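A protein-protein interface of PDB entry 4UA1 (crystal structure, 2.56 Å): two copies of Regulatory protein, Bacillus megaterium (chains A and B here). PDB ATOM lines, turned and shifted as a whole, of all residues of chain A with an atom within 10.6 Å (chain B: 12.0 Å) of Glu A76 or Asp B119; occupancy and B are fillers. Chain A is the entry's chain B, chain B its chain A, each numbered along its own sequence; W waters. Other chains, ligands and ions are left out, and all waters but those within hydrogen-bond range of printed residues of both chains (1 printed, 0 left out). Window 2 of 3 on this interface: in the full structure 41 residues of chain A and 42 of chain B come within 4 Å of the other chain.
O of Pro B115 sits at hydrogen-bond distance from NZ of Lys B118, 2.7 Å away.
O of Glu B116 is in hydrogen-bond range of NZ of Lys B118.
OD1 of Asn B117 lies within hydrogen-bond range of N of Asp B119 (3.1 Å).
The side-chain sulfur (SG) of Cys B123 sits close to the backbone NH (N) of Ile B126 (3.8 Å).
The side-chain amino group of Lys A78 lies within hydrogen-bond range of the backbone carbonyl oxygen of Asp A73 (3.4 Å).
The side-chain amino group (NZ) of Lys A78 sits at hydrogen-bond distance from the backbone carbonyl oxygen (O) of Asp A75 (2.7 Å).
No position is printed for both chains.
Of the 18 pairs that touch across the chains among the printed residues, none has its exchanged pair printed and touching as well.
The backbone carbonyl oxygen (O) of Lys B118 sits at hydrogen-bond distance from the backbone NH (N) of Arg A80 (3.1 Å).
N of Lys A78 sits at hydrogen-bond distance from O of Ile B120 (2.8 Å).
N of Cys A79 is in hydrogen-bond range of O of Ile B120 (3.2 Å).
OE1 of Glu A76 sits close to OD2 of Asp B119 (3.2 Å).
O of Ile B120 sits close to O of Glu A76 (3.4 Å).
Among the printed residues, merely in contact across the chains: Ala A77 with Asp B119 (3.4 Å), Cys A79 with Glu B122 (3.5 Å), Ala A77 with Lys B118 (3.5 Å), Cys A79 with Lys B118 (3.5 Å), Lys A78 with Tyr B121 (3.6 Å), Cys A79 with Cys B123 (3.6 Å), Tyr A83 with Lys B118 (3.6 Å), Met A82 with Cys B123 (3.6 Å), Met A82 with Ile B126 (3.6 Å), Ala A77 with Ile B120 (3.7 Å), Cys A79 with Pro B115 (3.8 Å), Cys A79 with Cys B114 (3.9 Å) and Val A72 with Ile B126 (3.98 Å).
Glu A76 touches just these residues of chain B: Asp B119 and Ile B120.
Asp B119 touches just these residues of chain A: Glu A76 (3.2 Å) and Ala A77 (3.4 Å).
Lys A78 touches two residues of chain B.
Cys A79 touches six residues of chain B.
No residue of chain A comes within 4 Å of Asn B117.
Ile B120 touches just these residues of chain A: Glu A76 (3.4 Å), Ala A77 (3.7 Å), Lys A78 (2.8 Å) and Cys A79 (3.2 Å).
Of the printed residues of chain A, Cys B123 touches Cys A79 (3.6 Å) and Met A82 (3.6 Å).
Of the printed residues of chain B, Met A82 touches Cys B123 and Ile B126.
Printed residues of chain A within 4 Å of Ile B126: Val A72 and Met A82.
The nearest residue of chain B that does not touch Glu A76 is Tyr B121 (4.2 Å).
The nearest printed residue of chain A that does not touch Tyr B121 is Glu A76 (4.2 Å).
Water W1 lies within hydrogen-bond range of NZ of Lys B118 (3.0 Å) and OH of Tyr A83 (3.4 Å).
Printed residues of chain A that touch a printed residue of chain B: Val A72, Glu A76, Ala A77, Lys A78, Cys A79, Arg A80, Met A82 and Tyr A83.
Hydrophobic or aromatic side chains of chain A within 4 Å of the printed part of chain B: Val A72, Ala A77, Met A82 and Tyr A83.
Hydrophobic or aromatic side chains of chain B that line the printed part of chain A: Pro B115, Ile B120, Tyr B121 and Ile B126.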
ATOM      1  N   LEU A  69      12.349   1.585  -6.413  1.00  0.00           N
ATOM      2  CA  LEU A  69      13.746   1.300  -6.186  1.00  0.00           C
ATOM      3  C   LEU A  69      14.234   1.863  -4.851  1.00  0.00           C
ATOM      4  O   LEU A  69      15.031   1.222  -4.168  1.00  0.00           O
ATOM      5  CB  LEU A  69      14.598   1.836  -7.337  1.00  0.00           C
ATOM      6  CG  LEU A  69      14.680   0.982  -8.606  1.00  0.00           C
ATOM      7  CD1 LEU A  69      15.553   1.674  -9.650  1.00  0.00           C
ATOM      8  CD2 LEU A  69      15.230  -0.405  -8.267  1.00  0.00           C
ATOM      9  N   GLY A  70      13.739   3.037  -4.461  1.00  0.00           N
ATOM     10  CA  GLY A  70      14.103   3.575  -3.160  1.00  0.00           C
ATOM     11  C   GLY A  70      13.699   2.662  -2.020  1.00  0.00           C
ATOM     12  O   GLY A  70      14.495   2.353  -1.106  1.00  0.00           O
ATOM     13  N   VAL A  71      12.445   2.227  -2.080  1.00  0.00           N
ATOM     14  CA  VAL A  71      11.878   1.333  -1.077  1.00  0.00           C
ATOM     15  C   VAL A  71      12.601  -0.019  -1.027  1.00  0.00           C
ATOM     16  O   VAL A  71      13.095  -0.429   0.029  1.00  0.00           O
ATOM     17  CB  VAL A  71      10.365   1.130  -1.327  1.00  0.00           C
ATOM     18  CG1 VAL A  71       9.775   0.145  -0.354  1.00  0.00           C
ATOM     19  CG2 VAL A  71       9.651   2.463  -1.200  1.00  0.00           C
ATOM     20  N   VAL A  72      12.694  -0.708  -2.159  1.00  0.00           N
ATOM     21  CA  VAL A  72      13.322  -2.023  -2.146  1.00  0.00           C
ATOM     22  C   VAL A  72      14.769  -1.906  -1.679  1.00  0.00           C
ATOM     23  O   VAL A  72      15.217  -2.678  -0.834  1.00  0.00           O
ATOM     24  CB  VAL A  72      13.304  -2.716  -3.534  1.00  0.00           C
ATOM     25  CG1 VAL A  72      13.981  -4.080  -3.447  1.00  0.00           C
ATOM     26  CG2 VAL A  72      11.879  -2.855  -4.060  1.00  0.00           C
ATOM     27  N   ASP A  73      15.489  -0.909  -2.179  1.00  0.00           N
ATOM     28  CA  ASP A  73      16.879  -0.725  -1.757  1.00  0.00           C
ATOM     29  C   ASP A  73      17.007  -0.476  -0.257  1.00  0.00           C
ATOM     30  O   ASP A  73      17.974  -0.913   0.357  1.00  0.00           O
ATOM     31  CB  ASP A  73      17.537   0.431  -2.515  1.00  0.00           C
ATOM     32  CG  ASP A  73      17.794   0.100  -3.990  1.00  0.00           C
ATOM     33  OD1 ASP A  73      17.754  -1.104  -4.351  1.00  0.00           O
ATOM     34  OD2 ASP A  73      18.014   1.049  -4.793  1.00  0.00           O
ATOM     35  N   ARG A  74      16.054   0.214   0.362  1.00  0.00           N
ATOM     36  CA  ARG A  74      16.274   0.481   1.781  1.00  0.00           C
ATOM     37  C   ARG A  74      15.633  -0.498   2.785  1.00  0.00           C
ATOM     38  O   ARG A  74      15.852  -0.364   3.980  1.00  0.00           O
ATOM     39  CB  ARG A  74      15.823   1.908   2.075  1.00  0.00           C
ATOM     40  CG  ARG A  74      16.689   2.905   1.311  1.00  0.00           C
ATOM     41  CD  ARG A  74      16.391   4.360   1.603  1.00  0.00           C
ATOM     42  NE  ARG A  74      16.671   5.152   0.406  1.00  0.00           N
ATOM     43  CZ  ARG A  74      16.252   6.401   0.207  1.00  0.00           C
ATOM     44  NH1 ARG A  74      15.538   7.031   1.134  1.00  0.00           N
ATOM     45  NH2 ARG A  74      16.558   7.030  -0.923  1.00  0.00           N
ATOM     46  N   ASP A  75      14.958  -1.546   2.324  1.00  0.00           N
ATOM     47  CA  ASP A  75      14.151  -2.361   3.233  1.00  0.00           C
ATOM     48  C   ASP A  75      14.686  -3.758   3.473  1.00  0.00           C
ATOM     49  O   ASP A  75      15.435  -4.298   2.663  1.00  0.00           O
ATOM     50  CB  ASP A  75      12.704  -2.496   2.727  1.00  0.00           C
ATOM     51  CG  ASP A  75      11.798  -1.320   3.143  1.00  0.00           C
ATOM     52  OD1 ASP A  75      12.246  -0.451   3.925  1.00  0.00           O
ATOM     53  OD2 ASP A  75      10.628  -1.278   2.701  1.00  0.00           O
ATOM     54  N   GLU A  76      14.303  -4.332   4.610  1.00  0.00           N
ATOM     55  CA  GLU A  76      14.651  -5.707   4.895  1.00  0.00           C
ATOM     56  C   GLU A  76      13.822  -6.670   4.042  1.00  0.00           C
ATOM     57  O   GLU A  76      14.365  -7.582   3.424  1.00  0.00           O
ATOM     58  CB  GLU A  76      14.482  -6.011   6.392  1.00  0.00           C
ATOM     59  CG  GLU A  76      14.692  -7.475   6.782  1.00  0.00           C
ATOM     60  CD  GLU A  76      14.687  -7.687   8.293  1.00  0.00           C
ATOM     61  OE1 GLU A  76      13.886  -8.517   8.780  1.00  0.00           O
ATOM     62  OE2 GLU A  76      15.498  -7.032   8.993  1.00  0.00           O
ATOM     63  N   ALA A  77      12.515  -6.483   3.973  1.00  0.00           N
ATOM     64  CA  ALA A  77      11.779  -7.460   3.195  1.00  0.00           C
ATOM     65  C   ALA A  77      11.632  -6.939   1.783  1.00  0.00           C
ATOM     66  O   ALA A  77      10.660  -6.263   1.449  1.00  0.00           O
ATOM     67  CB  ALA A  77      10.423  -7.715   3.818  1.00  0.00           C
ATOM     68  N   LYS A  78      12.546  -7.366   0.921  1.00  0.00           N
ATOM     69  CA  LYS A  78      12.575  -6.829  -0.430  1.00  0.00           C
ATOM     70  C   LYS A  78      11.552  -7.576  -1.265  1.00  0.00           C
ATOM     71  O   LYS A  78      10.833  -6.993  -2.062  1.00  0.00           O
ATOM     72  CB  LYS A  78      13.974  -6.919  -1.030  1.00  0.00           C
ATOM     73  CG  LYS A  78      15.015  -6.221  -0.214  1.00  0.00           C
ATOM     74  CD  LYS A  78      16.333  -6.151  -0.976  1.00  0.00           C
ATOM     75  CE  LYS A  78      17.443  -5.537  -0.110  1.00  0.00           C
ATOM     76  NZ  LYS A  78      17.033  -4.224   0.473  1.00  0.00           N
ATOM     77  N   CYS A  79      11.489  -8.883  -1.062  1.00  0.00           N
ATOM     78  CA  CYS A  79      10.512  -9.695  -1.736  1.00  0.00           C
ATOM     79  C   CYS A  79       9.083  -9.189  -1.455  1.00  0.00           C
ATOM     80  O   CYS A  79       8.279  -9.035  -2.377  1.00  0.00           O
ATOM     81  CB  CYS A  79      10.688 -11.147  -1.309  1.00  0.00           C
ATOM     82  SG  CYS A  79       9.435 -12.249  -1.935  1.00  0.00           S
ATOM     83  N   ARG A  80       8.781  -8.884  -0.195  1.00  0.00           N
ATOM     84  CA  ARG A  80       7.449  -8.390   0.144  1.00  0.00           C
ATOM     85  C   ARG A  80       7.144  -7.054  -0.568  1.00  0.00           C
ATOM     86  O   ARG A  80       6.038  -6.855  -1.101  1.00  0.00           O
ATOM     87  CB  ARG A  80       7.306  -8.228   1.668  1.00  0.00           C
ATOM     88  CG  ARG A  80       5.956  -7.690   2.120  1.00  0.00           C
ATOM     89  CD  ARG A  80       6.036  -7.163   3.543  1.00  0.00           C
ATOM     90  NE  ARG A  80       6.885  -5.974   3.570  1.00  0.00           N
ATOM     91  CZ  ARG A  80       7.388  -5.425   4.674  1.00  0.00           C
ATOM     92  NH1 ARG A  80       7.126  -5.967   5.860  1.00  0.00           N
ATOM     93  NH2 ARG A  80       8.162  -4.336   4.584  1.00  0.00           N
ATOM     94  N   ASP A  81       8.128  -6.149  -0.559  1.00  0.00           N
ATOM     95  CA  ASP A  81       7.977  -4.844  -1.180  1.00  0.00           C
ATOM     96  C   ASP A  81       7.629  -5.008  -2.630  1.00  0.00           C
ATOM     97  O   ASP A  81       6.649  -4.459  -3.135  1.00  0.00           O
ATOM     98  CB  ASP A  81       9.264  -4.019  -1.073  1.00  0.00           C
ATOM     99  CG  ASP A  81       9.511  -3.468   0.323  1.00  0.00           C
ATOM    100  OD1 ASP A  81       8.573  -3.394   1.148  1.00  0.00           O
ATOM    101  OD2 ASP A  81      10.672  -3.100   0.595  1.00  0.00           O
ATOM    102  N   MET A  82       8.449  -5.786  -3.301  1.00  0.00           N
ATOM    103  CA  MET A  82       8.302  -5.954  -4.721  1.00  0.00           C
ATOM    104  C   MET A  82       6.961  -6.613  -5.070  1.00  0.00           C
ATOM    105  O   MET A  82       6.301  -6.233  -6.041  1.00  0.00           O
ATOM    106  CB  MET A  82       9.472  -6.759  -5.261  1.00  0.00           C
ATOM    107  CG  MET A  82       9.572  -6.628  -6.749  1.00  0.00           C
ATOM    108  SD  MET A  82       9.702  -4.917  -7.248  1.00  0.00           S
ATOM    109  CE  MET A  82       9.191  -5.089  -8.951  1.00  0.00           C
ATOM    110  N   TYR A  83       6.553  -7.566  -4.237  1.00  0.00           N
ATOM    111  CA  TYR A  83       5.266  -8.231  -4.366  1.00  0.00           C
ATOM    112  C   TYR A  83       4.111  -7.238  -4.333  1.00  0.00           C
ATOM    113  O   TYR A  83       3.208  -7.248  -5.209  1.00  0.00           O
ATOM    114  CB  TYR A  83       5.149  -9.272  -3.252  1.00  0.00           C
ATOM    115  CG  TYR A  83       3.867 -10.074  -3.194  1.00  0.00           C
ATOM    116  CD1 TYR A  83       3.628 -11.114  -4.086  1.00  0.00           C
ATOM    117  CD2 TYR A  83       2.935  -9.854  -2.175  1.00  0.00           C
ATOM    118  CE1 TYR A  83       2.467 -11.865  -4.001  1.00  0.00           C
ATOM    119  CE2 TYR A  83       1.780 -10.605  -2.079  1.00  0.00           C
ATOM    120  CZ  TYR A  83       1.550 -11.617  -2.987  1.00  0.00           C
ATOM    121  OH  TYR A  83       0.399 -12.381  -2.885  1.00  0.00           O
ATOM    122  N   ASP A  84       4.141  -6.400  -3.300  1.00  0.00           N
ATOM    123  CA  ASP A  84       3.171  -5.312  -3.129  1.00  0.00           C
ATOM    124  C   ASP A  84       3.097  -4.350  -4.311  1.00  0.00           C
ATOM    125  O   ASP A  84       2.005  -4.034  -4.784  1.00  0.00           O
ATOM    126  CB  ASP A  84       3.491  -4.527  -1.870  1.00  0.00           C
ATOM    127  CG  ASP A  84       3.157  -5.294  -0.650  1.00  0.00           C
ATOM    128  OD1 ASP A  84       2.363  -6.242  -0.784  1.00  0.00           O
ATOM    129  OD2 ASP A  84       3.649  -4.951   0.437  1.00  0.00           O
ATOM    130  N   ARG B 113       5.301 -16.183  -8.428  1.00  0.00           N
ATOM    131  CA  ARG B 113       6.600 -16.777  -8.062  1.00  0.00           C
ATOM    132  C   ARG B 113       7.073 -16.557  -6.591  1.00  0.00           C
ATOM    133  O   ARG B 113       7.974 -17.252  -6.115  1.00  0.00           O
ATOM    134  CB  ARG B 113       7.700 -16.244  -8.997  1.00  0.00           C
ATOM    135  CG  ARG B 113       7.526 -16.580 -10.470  1.00  0.00           C
ATOM    136  CD  ARG B 113       8.500 -15.747 -11.314  1.00  0.00           C
ATOM    137  NE  ARG B 113       8.362 -16.025 -12.738  1.00  0.00           N
ATOM    138  CZ  ARG B 113       9.104 -16.904 -13.404  1.00  0.00           C
ATOM    139  NH1 ARG B 113      10.054 -17.591 -12.772  1.00  0.00           N
ATOM    140  NH2 ARG B 113       8.901 -17.086 -14.703  1.00  0.00           N
ATOM    141  N   CYS B 114       6.522 -15.571  -5.893  1.00  0.00           N
ATOM    142  CA  CYS B 114       7.102 -15.182  -4.607  1.00  0.00           C
ATOM    143  C   CYS B 114       6.715 -16.220  -3.496  1.00  0.00           C
ATOM    144  O   CYS B 114       5.603 -16.767  -3.489  1.00  0.00           O
ATOM    145  CB  CYS B 114       6.689 -13.722  -4.290  1.00  0.00           C
ATOM    146  SG  CYS B 114       7.341 -12.475  -5.518  1.00  0.00           S
ATOM    147  N   PRO B 115       7.651 -16.525  -2.568  1.00  0.00           N
ATOM    148  CA  PRO B 115       7.367 -17.500  -1.497  1.00  0.00           C
ATOM    149  C   PRO B 115       6.367 -16.962  -0.458  1.00  0.00           C
ATOM    150  O   PRO B 115       6.067 -15.756  -0.456  1.00  0.00           O
ATOM    151  CB  PRO B 115       8.739 -17.732  -0.849  1.00  0.00           C
ATOM    152  CG  PRO B 115       9.509 -16.497  -1.126  1.00  0.00           C
ATOM    153  CD  PRO B 115       9.033 -16.007  -2.493  1.00  0.00           C
ATOM    154  N   GLU B 116       5.858 -17.843   0.403  1.00  0.00           N
ATOM    155  CA  GLU B 116       4.916 -17.446   1.446  1.00  0.00           C
ATOM    156  C   GLU B 116       5.545 -16.442   2.399  1.00  0.00           C
ATOM    157  O   GLU B 116       4.942 -15.400   2.676  1.00  0.00           O
ATOM    158  CB  GLU B 116       4.411 -18.659   2.226  1.00  0.00           C
ATOM    159  CG  GLU B 116       3.614 -19.610   1.358  1.00  0.00           C
ATOM    160  CD  GLU B 116       2.695 -20.510   2.146  1.00  0.00           C
ATOM    161  OE1 GLU B 116       2.992 -20.749   3.347  1.00  0.00           O
ATOM    162  OE2 GLU B 116       1.676 -20.970   1.561  1.00  0.00           O
ATOM    163  N   ASN B 117       6.759 -16.733   2.882  1.00  0.00           N
ATOM    164  CA  ASN B 117       7.451 -15.755   3.708  1.00  0.00           C
ATOM    165  C   ASN B 117       8.341 -14.828   2.866  1.00  0.00           C
ATOM    166  O   ASN B 117       9.411 -15.184   2.379  1.00  0.00           O
ATOM    167  CB  ASN B 117       8.275 -16.449   4.783  1.00  0.00           C
ATOM    168  CG  ASN B 117       9.150 -15.481   5.560  1.00  0.00           C
ATOM    169  OD1 ASN B 117       8.801 -14.306   5.749  1.00  0.00           O
ATOM    170  ND2 ASN B 117      10.297 -15.962   6.002  1.00  0.00           N
ATOM    171  N   LYS B 118       7.877 -13.601   2.751  1.00  0.00           N
ATOM    172  CA  LYS B 118       8.447 -12.613   1.868  1.00  0.00           C
ATOM    173  C   LYS B 118       9.382 -11.688   2.612  1.00  0.00           C
ATOM    174  O   LYS B 118       9.807 -10.674   2.062  1.00  0.00           O
ATOM    175  CB  LYS B 118       7.334 -11.847   1.166  1.00  0.00           C
ATOM    176  CG  LYS B 118       6.389 -12.785   0.415  1.00  0.00           C
ATOM    177  CD  LYS B 118       5.377 -12.037  -0.453  1.00  0.00           C
ATOM    178  CE  LYS B 118       4.468 -13.001  -1.179  1.00  0.00           C
ATOM    179  NZ  LYS B 118       3.974 -14.030  -0.236  1.00  0.00           N
ATOM    180  N   ASP B 119       9.685 -11.991   3.872  1.00  0.00           N
ATOM    181  CA  ASP B 119      10.626 -11.110   4.520  1.00  0.00           C
ATOM    182  C   ASP B 119      12.016 -11.657   4.247  1.00  0.00           C
ATOM    183  O   ASP B 119      12.614 -12.307   5.082  1.00  0.00           O
ATOM    184  CB  ASP B 119      10.345 -11.084   6.022  1.00  0.00           C
ATOM    185  CG  ASP B 119      11.383 -10.304   6.805  1.00  0.00           C
ATOM    186  OD1 ASP B 119      12.051  -9.408   6.233  1.00  0.00           O
ATOM    187  OD2 ASP B 119      11.546 -10.613   8.003  1.00  0.00           O
ATOM    188  N   ILE B 120      12.580 -11.219   3.129  1.00  0.00           N
ATOM    189  CA  ILE B 120      13.848 -11.742   2.603  1.00  0.00           C
ATOM    190  C   ILE B 120      14.416 -10.777   1.575  1.00  0.00           C
ATOM    191  O   ILE B 120      13.706  -9.891   1.040  1.00  0.00           O
ATOM    192  CB  ILE B 120      13.713 -13.135   1.935  1.00  0.00           C
ATOM    193  CG1 ILE B 120      12.566 -13.137   0.916  1.00  0.00           C
ATOM    194  CG2 ILE B 120      13.541 -14.244   2.978  1.00  0.00           C
ATOM    195  CD1 ILE B 120      12.377 -14.455   0.245  1.00  0.00           C
ATOM    196  N   TYR B 121      15.700 -10.974   1.310  1.00  0.00           N
ATOM    197  CA  TYR B 121      16.487 -10.222   0.352  1.00  0.00           C
ATOM    198  C   TYR B 121      16.221 -10.613  -1.096  1.00  0.00           C
ATOM    199  O   TYR B 121      16.147  -9.758  -1.977  1.00  0.00           O
ATOM    200  CB  TYR B 121      17.957 -10.441   0.686  1.00  0.00           C
ATOM    201  CG  TYR B 121      18.919  -9.546  -0.047  1.00  0.00           C
ATOM    202  CD1 TYR B 121      19.447  -8.413   0.568  1.00  0.00           C
ATOM    203  CD2 TYR B 121      19.329  -9.847  -1.345  1.00  0.00           C
ATOM    204  CE1 TYR B 121      20.349  -7.589  -0.106  1.00  0.00           C
ATOM    205  CE2 TYR B 121      20.231  -9.039  -2.019  1.00  0.00           C
ATOM    206  CZ  TYR B 121      20.735  -7.914  -1.398  1.00  0.00           C
ATOM    207  OH  TYR B 121      21.623  -7.115  -2.085  1.00  0.00           O
ATOM    208  N   GLU B 122      16.033 -11.909  -1.310  1.00  0.00           N
ATOM    209  CA  GLU B 122      15.863 -12.500  -2.636  1.00  0.00           C
ATOM    210  C   GLU B 122      14.428 -12.335  -3.096  1.00  0.00           C
ATOM    211  O   GLU B 122      13.521 -12.849  -2.443  1.00  0.00           O
ATOM    212  CB  GLU B 122      16.133 -14.014  -2.630  1.00  0.00           C
ATOM    213  CG  GLU B 122      17.426 -14.554  -2.044  1.00  0.00           C
ATOM    214  CD  GLU B 122      17.255 -14.978  -0.576  1.00  0.00           C
ATOM    215  OE1 GLU B 122      17.956 -15.912  -0.123  1.00  0.00           O
ATOM    216  OE2 GLU B 122      16.348 -14.456   0.102  1.00  0.00           O
ATOM    217  N   CYS B 123      14.184 -11.623  -4.186  1.00  0.00           N
ATOM    218  CA  CYS B 123      12.823 -11.615  -4.738  1.00  0.00           C
ATOM    219  C   CYS B 123      12.812 -12.255  -6.130  1.00  0.00           C
ATOM    220  O   CYS B 123      13.455 -11.759  -7.065  1.00  0.00           O
ATOM    221  CB  CYS B 123      12.244 -10.205  -4.803  1.00  0.00           C
ATOM    222  SG  CYS B 123      10.626 -10.115  -5.658  1.00  0.00           S
ATOM    223  N   PRO B 124      12.086 -13.357  -6.274  1.00  0.00           N
ATOM    224  CA  PRO B 124      11.952 -14.026  -7.575  1.00  0.00           C
ATOM    225  C   PRO B 124      11.478 -13.101  -8.699  1.00  0.00           C
ATOM    226  O   PRO B 124      11.841 -13.313  -9.849  1.00  0.00           O
ATOM    227  CB  PRO B 124      10.899 -15.104  -7.305  1.00  0.00           C
ATOM    228  CG  PRO B 124      10.976 -15.341  -5.821  1.00  0.00           C
ATOM    229  CD  PRO B 124      11.351 -14.036  -5.200  1.00  0.00           C
ATOM    230  N   ILE B 126      12.199  -9.791  -9.100  1.00  0.00           N
ATOM    231  CA  ILE B 126      13.349  -9.018  -9.480  1.00  0.00           C
ATOM    232  C   ILE B 126      14.357  -9.897 -10.223  1.00  0.00           C
ATOM    233  O   ILE B 126      14.883  -9.509 -11.271  1.00  0.00           O
ATOM    234  CB  ILE B 126      13.986  -8.371  -8.239  1.00  0.00           C
ATOM    235  CG1 ILE B 126      12.969  -7.417  -7.600  1.00  0.00           C
ATOM    236  CG2 ILE B 126      15.273  -7.610  -8.611  1.00  0.00           C
ATOM    237  CD1 ILE B 126      13.392  -6.852  -6.238  1.00  0.00           C
HETATM  238  O   HOH W   1       1.854 -15.290  -2.025  1.00  0.00           O
